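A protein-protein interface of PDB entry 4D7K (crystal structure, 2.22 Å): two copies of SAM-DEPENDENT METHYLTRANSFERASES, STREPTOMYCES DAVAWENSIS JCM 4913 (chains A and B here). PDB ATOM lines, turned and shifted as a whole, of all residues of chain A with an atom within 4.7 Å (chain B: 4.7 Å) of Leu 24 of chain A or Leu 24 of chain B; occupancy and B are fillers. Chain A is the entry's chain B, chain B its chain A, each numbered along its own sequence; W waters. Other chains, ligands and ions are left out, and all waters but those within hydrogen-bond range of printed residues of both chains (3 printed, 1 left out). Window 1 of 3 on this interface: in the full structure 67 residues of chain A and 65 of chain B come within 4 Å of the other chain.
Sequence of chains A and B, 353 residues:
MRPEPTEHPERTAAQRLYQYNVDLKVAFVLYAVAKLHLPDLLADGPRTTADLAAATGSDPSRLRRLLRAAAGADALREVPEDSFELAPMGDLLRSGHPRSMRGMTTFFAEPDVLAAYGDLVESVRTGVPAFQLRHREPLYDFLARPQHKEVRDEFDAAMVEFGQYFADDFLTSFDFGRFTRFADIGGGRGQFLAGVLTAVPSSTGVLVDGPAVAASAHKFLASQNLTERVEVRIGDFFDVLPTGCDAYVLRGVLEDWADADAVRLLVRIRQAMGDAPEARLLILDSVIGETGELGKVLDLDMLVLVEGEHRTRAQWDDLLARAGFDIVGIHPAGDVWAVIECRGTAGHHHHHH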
ATOM      1  N   TYR A  20      -8.164 -13.870 -11.538  1.00  0.00           N
ATOM      2  CA  TYR A  20      -9.065 -13.041 -12.338  1.00  0.00           C
ATOM      3  C   TYR A  20     -10.317 -13.818 -12.731  1.00  0.00           C
ATOM      4  O   TYR A  20     -11.408 -13.256 -12.797  1.00  0.00           O
ATOM      5  CB  TYR A  20      -8.370 -12.516 -13.597  1.00  0.00           C
ATOM      6  CG  TYR A  20      -7.444 -11.356 -13.338  1.00  0.00           C
ATOM      7  CD1 TYR A  20      -7.910 -10.199 -12.733  1.00  0.00           C
ATOM      8  CD2 TYR A  20      -6.106 -11.414 -13.704  1.00  0.00           C
ATOM      9  CE1 TYR A  20      -7.068  -9.133 -12.491  1.00  0.00           C
ATOM     10  CE2 TYR A  20      -5.254 -10.350 -13.468  1.00  0.00           C
ATOM     11  CZ  TYR A  20      -5.740  -9.215 -12.864  1.00  0.00           C
ATOM     12  OH  TYR A  20      -4.899  -8.155 -12.627  1.00  0.00           O
ATOM     13  N   ASN A  21     -10.147 -15.109 -12.999  1.00  0.00           N
ATOM     14  CA  ASN A  21     -11.270 -15.986 -13.312  1.00  0.00           C
ATOM     15  C   ASN A  21     -12.218 -16.111 -12.123  1.00  0.00           C
ATOM     16  O   ASN A  21     -13.436 -16.067 -12.277  1.00  0.00           O
ATOM     17  CB  ASN A  21     -10.764 -17.364 -13.734  1.00  0.00           C
ATOM     18  CG  ASN A  21     -11.875 -18.271 -14.226  1.00  0.00           C
ATOM     19  OD1 ASN A  21     -12.322 -19.172 -13.514  1.00  0.00           O
ATOM     20  ND2 ASN A  21     -12.319 -18.043 -15.455  1.00  0.00           N
ATOM     21  N   VAL A  22     -11.646 -16.253 -10.932  1.00  0.00           N
ATOM     22  CA  VAL A  22     -12.432 -16.365  -9.707  1.00  0.00           C
ATOM     23  C   VAL A  22     -13.155 -15.062  -9.386  1.00  0.00           C
ATOM     24  O   VAL A  22     -14.335 -15.065  -9.033  1.00  0.00           O
ATOM     25  CB  VAL A  22     -11.539 -16.769  -8.517  1.00  0.00           C
ATOM     26  CG1 VAL A  22     -12.275 -16.602  -7.179  1.00  0.00           C
ATOM     27  CG2 VAL A  22     -11.057 -18.194  -8.700  1.00  0.00           C
ATOM     28  N   ASP A  23     -12.449 -13.945  -9.520  1.00  0.00           N
ATOM     29  CA  ASP A  23     -13.021 -12.646  -9.195  1.00  0.00           C
ATOM     30  C   ASP A  23     -14.168 -12.264 -10.140  1.00  0.00           C
ATOM     31  O   ASP A  23     -15.109 -11.573  -9.744  1.00  0.00           O
ATOM     32  CB  ASP A  23     -11.928 -11.575  -9.214  1.00  0.00           C
ATOM     33  CG  ASP A  23     -10.931 -11.737  -8.069  1.00  0.00           C
ATOM     34  OD1 ASP A  23     -11.133 -12.622  -7.211  1.00  0.00           O
ATOM     35  OD2 ASP A  23      -9.946 -10.971  -8.020  1.00  0.00           O
ATOM     36  N   LEU A  24     -14.081 -12.725 -11.385  1.00  0.00           N
ATOM     37  CA  LEU A  24     -15.165 -12.575 -12.349  1.00  0.00           C
ATOM     38  C   LEU A  24     -16.465 -13.191 -11.811  1.00  0.00           C
ATOM     39  O   LEU A  24     -17.538 -12.599 -11.927  1.00  0.00           O
ATOM     40  CB  LEU A  24     -14.766 -13.218 -13.683  1.00  0.00           C
ATOM     41  CG  LEU A  24     -15.770 -13.193 -14.830  1.00  0.00           C
ATOM     42  CD1 LEU A  24     -16.235 -11.778 -15.072  1.00  0.00           C
ATOM     43  CD2 LEU A  24     -15.158 -13.789 -16.101  1.00  0.00           C
ATOM     44  N   LYS A  25     -16.358 -14.369 -11.202  1.00  0.00           N
ATOM     45  CA  LYS A  25     -17.511 -15.036 -10.601  1.00  0.00           C
ATOM     46  C   LYS A  25     -18.031 -14.294  -9.374  1.00  0.00           C
ATOM     47  O   LYS A  25     -19.239 -14.149  -9.194  1.00  0.00           O
ATOM     48  CB  LYS A  25     -17.149 -16.470 -10.220  1.00  0.00           C
ATOM     49  CG  LYS A  25     -16.530 -17.266 -11.353  1.00  0.00           C
ATOM     50  CD  LYS A  25     -16.121 -18.651 -10.879  1.00  0.00           C
ATOM     51  CE  LYS A  25     -15.207 -19.324 -11.884  1.00  0.00           C
ATOM     52  NZ  LYS A  25     -15.796 -19.333 -13.254  1.00  0.00           N
ATOM     53  N   VAL A  26     -17.120 -13.831  -8.523  1.00  0.00           N
ATOM     54  CA  VAL A  26     -17.512 -13.053  -7.352  1.00  0.00           C
ATOM     55  C   VAL A  26     -18.285 -11.804  -7.781  1.00  0.00           C
ATOM     56  O   VAL A  26     -19.276 -11.422  -7.150  1.00  0.00           O
ATOM     57  CB  VAL A  26     -16.283 -12.650  -6.494  1.00  0.00           C
ATOM     58  CG1 VAL A  26     -16.686 -11.661  -5.413  1.00  0.00           C
ATOM     59  CG2 VAL A  26     -15.646 -13.881  -5.859  1.00  0.00           C
ATOM     60  N   ALA A  27     -17.844 -11.187  -8.875  1.00  0.00           N
ATOM     61  CA  ALA A  27     -18.506 -10.007  -9.408  1.00  0.00           C
ATOM     62  C   ALA A  27     -19.967 -10.299  -9.761  1.00  0.00           C
ATOM     63  O   ALA A  27     -20.853  -9.498  -9.460  1.00  0.00           O
ATOM     64  CB  ALA A  27     -17.759  -9.486 -10.622  1.00  0.00           C
ATOM     65  N   PHE A  28     -20.218 -11.445 -10.387  1.00  0.00           N
ATOM     66  CA  PHE A  28     -21.591 -11.855 -10.696  1.00  0.00           C
ATOM     67  C   PHE A  28     -22.380 -12.162  -9.433  1.00  0.00           C
ATOM     68  O   PHE A  28     -23.574 -11.869  -9.347  1.00  0.00           O
ATOM     69  CB  PHE A  28     -21.603 -13.078 -11.615  1.00  0.00           C
ATOM     70  CG  PHE A  28     -21.311 -12.753 -13.043  1.00  0.00           C
ATOM     71  CD1 PHE A  28     -22.251 -12.089 -13.816  1.00  0.00           C
ATOM     72  CD2 PHE A  28     -20.101 -13.104 -13.616  1.00  0.00           C
ATOM     73  CE1 PHE A  28     -21.986 -11.782 -15.136  1.00  0.00           C
ATOM     74  CE2 PHE A  28     -19.828 -12.800 -14.935  1.00  0.00           C
ATOM     75  CZ  PHE A  28     -20.771 -12.138 -15.697  1.00  0.00           C
ATOM     76  N   PHE A 108     -22.139  -2.100 -13.835  1.00  0.00           N
ATOM     77  CA  PHE A 108     -21.166  -2.686 -14.757  1.00  0.00           C
ATOM     78  C   PHE A 108     -21.380  -4.179 -15.012  1.00  0.00           C
ATOM     79  O   PHE A 108     -20.710  -4.763 -15.863  1.00  0.00           O
ATOM     80  CB  PHE A 108     -19.742  -2.435 -14.244  1.00  0.00           C
ATOM     81  CG  PHE A 108     -19.325  -0.997 -14.344  1.00  0.00           C
ATOM     82  CD1 PHE A 108     -19.603  -0.109 -13.315  1.00  0.00           C
ATOM     83  CD2 PHE A 108     -18.695  -0.519 -15.486  1.00  0.00           C
ATOM     84  CE1 PHE A 108     -19.243   1.227 -13.414  1.00  0.00           C
ATOM     85  CE2 PHE A 108     -18.329   0.813 -15.592  1.00  0.00           C
ATOM     86  CZ  PHE A 108     -18.603   1.689 -14.555  1.00  0.00           C
ATOM     87  N   TYR B  20     -12.899  -5.353  -7.240  1.00  0.00           N
ATOM     88  CA  TYR B  20     -13.677  -6.284  -8.062  1.00  0.00           C
ATOM     89  C   TYR B  20     -14.160  -5.607  -9.340  1.00  0.00           C
ATOM     90  O   TYR B  20     -14.230  -6.236 -10.397  1.00  0.00           O
ATOM     91  CB  TYR B  20     -14.876  -6.849  -7.285  1.00  0.00           C
ATOM     92  CG  TYR B  20     -14.504  -7.948  -6.318  1.00  0.00           C
ATOM     93  CD1 TYR B  20     -13.858  -9.097  -6.763  1.00  0.00           C
ATOM     94  CD2 TYR B  20     -14.793  -7.841  -4.960  1.00  0.00           C
ATOM     95  CE1 TYR B  20     -13.506 -10.104  -5.894  1.00  0.00           C
ATOM     96  CE2 TYR B  20     -14.441  -8.852  -4.074  1.00  0.00           C
ATOM     97  CZ  TYR B  20     -13.797  -9.980  -4.553  1.00  0.00           C
ATOM     98  OH  TYR B  20     -13.447 -10.992  -3.696  1.00  0.00           O
ATOM     99  N   ASN B  21     -14.503  -4.326  -9.235  1.00  0.00           N
ATOM    100  CA  ASN B  21     -14.905  -3.534 -10.392  1.00  0.00           C
ATOM    101  C   ASN B  21     -13.759  -3.417 -11.394  1.00  0.00           C
ATOM    102  O   ASN B  21     -13.954  -3.560 -12.598  1.00  0.00           O
ATOM    103  CB  ASN B  21     -15.371  -2.146  -9.949  1.00  0.00           C
ATOM    104  CG  ASN B  21     -15.974  -1.338 -11.086  1.00  0.00           C
ATOM    105  OD1 ASN B  21     -15.327  -0.451 -11.645  1.00  0.00           O
ATOM    106  ND2 ASN B  21     -17.222  -1.637 -11.425  1.00  0.00           N
ATOM    107  N   VAL B  22     -12.558  -3.172 -10.879  1.00  0.00           N
ATOM    108  CA  VAL B  22     -11.364  -3.069 -11.706  1.00  0.00           C
ATOM    109  C   VAL B  22     -10.981  -4.405 -12.346  1.00  0.00           C
ATOM    110  O   VAL B  22     -10.697  -4.471 -13.542  1.00  0.00           O
ATOM    111  CB  VAL B  22     -10.175  -2.542 -10.881  1.00  0.00           C
ATOM    112  CG1 VAL B  22      -8.879  -2.619 -11.678  1.00  0.00           C
ATOM    113  CG2 VAL B  22     -10.450  -1.116 -10.410  1.00  0.00           C
ATOM    114  N   ASP B  23     -10.983  -5.472 -11.554  1.00  0.00           N
ATOM    115  CA  ASP B  23     -10.563  -6.774 -12.054  1.00  0.00           C
ATOM    116  C   ASP B  23     -11.572  -7.316 -13.077  1.00  0.00           C
ATOM    117  O   ASP B  23     -11.245  -8.170 -13.905  1.00  0.00           O
ATOM    118  CB  ASP B  23     -10.366  -7.753 -10.889  1.00  0.00           C
ATOM    119  CG  ASP B  23      -9.146  -7.406 -10.031  1.00  0.00           C
ATOM    120  OD1 ASP B  23      -8.555  -6.321 -10.233  1.00  0.00           O
ATOM    121  OD2 ASP B  23      -8.775  -8.211  -9.147  1.00  0.00           O
ATOM    122  N   LEU B  24     -12.792  -6.795 -13.025  1.00  0.00           N
ATOM    123  CA  LEU B  24     -13.801  -7.118 -14.019  1.00  0.00           C
ATOM    124  C   LEU B  24     -13.390  -6.549 -15.380  1.00  0.00           C
ATOM    125  O   LEU B  24     -13.413  -7.253 -16.386  1.00  0.00           O
ATOM    126  CB  LEU B  24     -15.166  -6.580 -13.582  1.00  0.00           C
ATOM    127  CG  LEU B  24     -16.358  -6.764 -14.516  1.00  0.00           C
ATOM    128  CD1 LEU B  24     -16.483  -8.203 -14.970  1.00  0.00           C
ATOM    129  CD2 LEU B  24     -17.619  -6.326 -13.804  1.00  0.00           C
ATOM    130  N   LYS B  25     -12.994  -5.280 -15.403  1.00  0.00           N
ATOM    131  CA  LYS B  25     -12.477  -4.657 -16.618  1.00  0.00           C
ATOM    132  C   LYS B  25     -11.226  -5.367 -17.143  1.00  0.00           C
ATOM    133  O   LYS B  25     -11.042  -5.509 -18.350  1.00  0.00           O
ATOM    134  CB  LYS B  25     -12.153  -3.184 -16.365  1.00  0.00           C
ATOM    135  CG  LYS B  25     -13.318  -2.347 -15.872  1.00  0.00           C
ATOM    136  CD  LYS B  25     -12.817  -0.983 -15.402  1.00  0.00           C
ATOM    137  CE  LYS B  25     -13.780  -0.332 -14.423  1.00  0.00           C
ATOM    138  NZ  LYS B  25     -15.127  -0.135 -15.022  1.00  0.00           N
ATOM    139  N   VAL B  26     -10.361  -5.800 -16.234  1.00  0.00           N
ATOM    140  CA  VAL B  26      -9.161  -6.520 -16.632  1.00  0.00           C
ATOM    141  C   VAL B  26      -9.526  -7.834 -17.329  1.00  0.00           C
ATOM    142  O   VAL B  26      -8.912  -8.203 -18.334  1.00  0.00           O
ATOM    143  CB  VAL B  26      -8.240  -6.799 -15.421  1.00  0.00           C
ATOM    144  CG1 VAL B  26      -7.121  -7.753 -15.803  1.00  0.00           C
ATOM    145  CG2 VAL B  26      -7.665  -5.489 -14.869  1.00  0.00           C
ATOM    146  N   ALA B  27     -10.537  -8.522 -16.803  1.00  0.00           N
ATOM    147  CA  ALA B  27     -10.989  -9.788 -17.378  1.00  0.00           C
ATOM    148  C   ALA B  27     -11.397  -9.614 -18.832  1.00  0.00           C
ATOM    149  O   ALA B  27     -11.110 -10.467 -19.677  1.00  0.00           O
ATOM    150  CB  ALA B  27     -12.144 -10.360 -16.578  1.00  0.00           C
ATOM    151  N   PHE B  28     -12.067  -8.504 -19.114  1.00  0.00           N
ATOM    152  CA  PHE B  28     -12.515  -8.211 -20.465  1.00  0.00           C
ATOM    153  C   PHE B  28     -11.344  -7.869 -21.366  1.00  0.00           C
ATOM    154  O   PHE B  28     -11.336  -8.230 -22.543  1.00  0.00           O
ATOM    155  CB  PHE B  28     -13.526  -7.065 -20.466  1.00  0.00           C
ATOM    156  CG  PHE B  28     -14.916  -7.486 -20.090  1.00  0.00           C
ATOM    157  CD1 PHE B  28     -15.662  -8.280 -20.944  1.00  0.00           C
ATOM    158  CD2 PHE B  28     -15.476  -7.083 -18.891  1.00  0.00           C
ATOM    159  CE1 PHE B  28     -16.947  -8.672 -20.603  1.00  0.00           C
ATOM    160  CE2 PHE B  28     -16.761  -7.464 -18.544  1.00  0.00           C
ATOM    161  CZ  PHE B  28     -17.498  -8.260 -19.400  1.00  0.00           C
ATOM    162  N   PHE B 108     -15.056 -18.216 -20.188  1.00  0.00           N
ATOM    163  CA  PHE B 108     -15.987 -17.619 -19.233  1.00  0.00           C
ATOM    164  C   PHE B 108     -16.334 -16.171 -19.564  1.00  0.00           C
ATOM    165  O   PHE B 108     -17.085 -15.524 -18.834  1.00  0.00           O
ATOM    166  CB  PHE B 108     -15.416 -17.717 -17.813  1.00  0.00           C
ATOM    167  CG  PHE B 108     -15.291 -19.127 -17.324  1.00  0.00           C
ATOM    168  CD1 PHE B 108     -16.383 -19.780 -16.773  1.00  0.00           C
ATOM    169  CD2 PHE B 108     -14.100 -19.817 -17.459  1.00  0.00           C
ATOM    170  CE1 PHE B 108     -16.282 -21.087 -16.344  1.00  0.00           C
ATOM    171  CE2 PHE B 108     -13.991 -21.126 -17.033  1.00  0.00           C
ATOM    172  CZ  PHE B 108     -15.083 -21.762 -16.472  1.00  0.00           C
HETATM  173  O   HOH W   1     -10.594  -8.379  -7.375  1.00  0.00           O
HETATM  174  O   HOH W   2     -11.854 -13.126  -4.290  1.00  0.00           O
HETATM  175  O   HOH W   3      -5.718  -5.923 -11.698  1.00  0.00           O
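OD2 of Asp 23 of chain A lies close to OD2 of Asp 23 of chain B, 3.2 Å away.
OD1 of Asn 21 of chain A sits close to NZ of Lys 25 of chain A (3.5 Å).
The side-chain amide oxygen of Asn 21 of chain B sits close to the side-chain amino group of Lys 25 of chain B (3.4 Å).
Among the printed residues, pairs that only touch across the chains: Asn 21 of chain A with Phe 108 of chain B (3.2 Å), Phe 108 of chain A with Lys 25 of chain B (3.4 Å), Phe 108 of chain A with Asn 21 of chain B (3.4 Å), Val 26 of chain A with Tyr 20 of chain B (3.5 Å), Tyr 20 of chain A with Val 26 of chain B (3.6 Å), Leu 24 of chain A with Leu 24 of chain B (3.6 Å), Lys 25 of chain A with Phe 108 of chain B (3.6 Å), Tyr 20 of chain A with Asp 23 of chain B (3.7 Å), Asp 23 of chain A with Tyr 20 of chain B (3.7 Å) and Leu 24 of chain A with Phe 108 of chain B (3.8 Å).
Leu 24 of chain A touches just these residues of chain B: Leu 24 and Phe 108.
Of chain A, only Leu 24 (3.6 Å) comes within 4 Å of Leu 24 of chain B.
Of the printed residues of chain A, Val 26 of chain B touches Tyr 20.
Of the printed residues of chain B, Asp 23 of chain A touches Tyr 20 (3.7 Å) and Asp 23 (3.2 Å).
Of the printed residues of chain B, Val 26 of chain A touches Tyr 20 (3.5 Å).
The nearest printed residue of chain A that does not touch Tyr 20 of chain B is Ala 27 of chain A (4.8 Å).
Hydrophobic or aromatic side chains of chain B within 4 Å of the printed part of chain A: Tyr 20, Leu 24, Val 26 and Phe 108.
Among the printed residues, 11 pairs touch across the chains.
Among the printed residues, no Asp or Glu carboxylate lies within 4 Å of a Lys or Arg side-chain nitrogen of the other chain.
Tyr 20 of chain A touches Asp 23 of chain B, and with the chains exchanged Asp 23 of chain A touches Tyr 20 of chain B.
Asn 21 of chain A touches Phe 108 of chain B, and with the chains exchanged Phe 108 of chain A touches Asn 21 of chain B.
Asp 23 of chain A touches its own counterpart, Asp 23 of chain B.
Leu 24 of chain B touches its own counterpart, Leu 24 of chain A.
Water W1 lies within hydrogen-bond range of the side-chain carboxylate of Asp 23 of chain B (2.5 Å) and the side-chain carboxylate of Asp 23 of chain A (2.7 Å).
Water W3 lies within hydrogen-bond range of OH of Tyr 20 of chain A (2.6 Å) and OD1 of Asp 23 of chain B (3.2 Å).
Water W2 lies within hydrogen-bond range of OH of Tyr 20 of chain B (2.7 Å) and OD1 of Asp 23 of chain A (3.1 Å).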
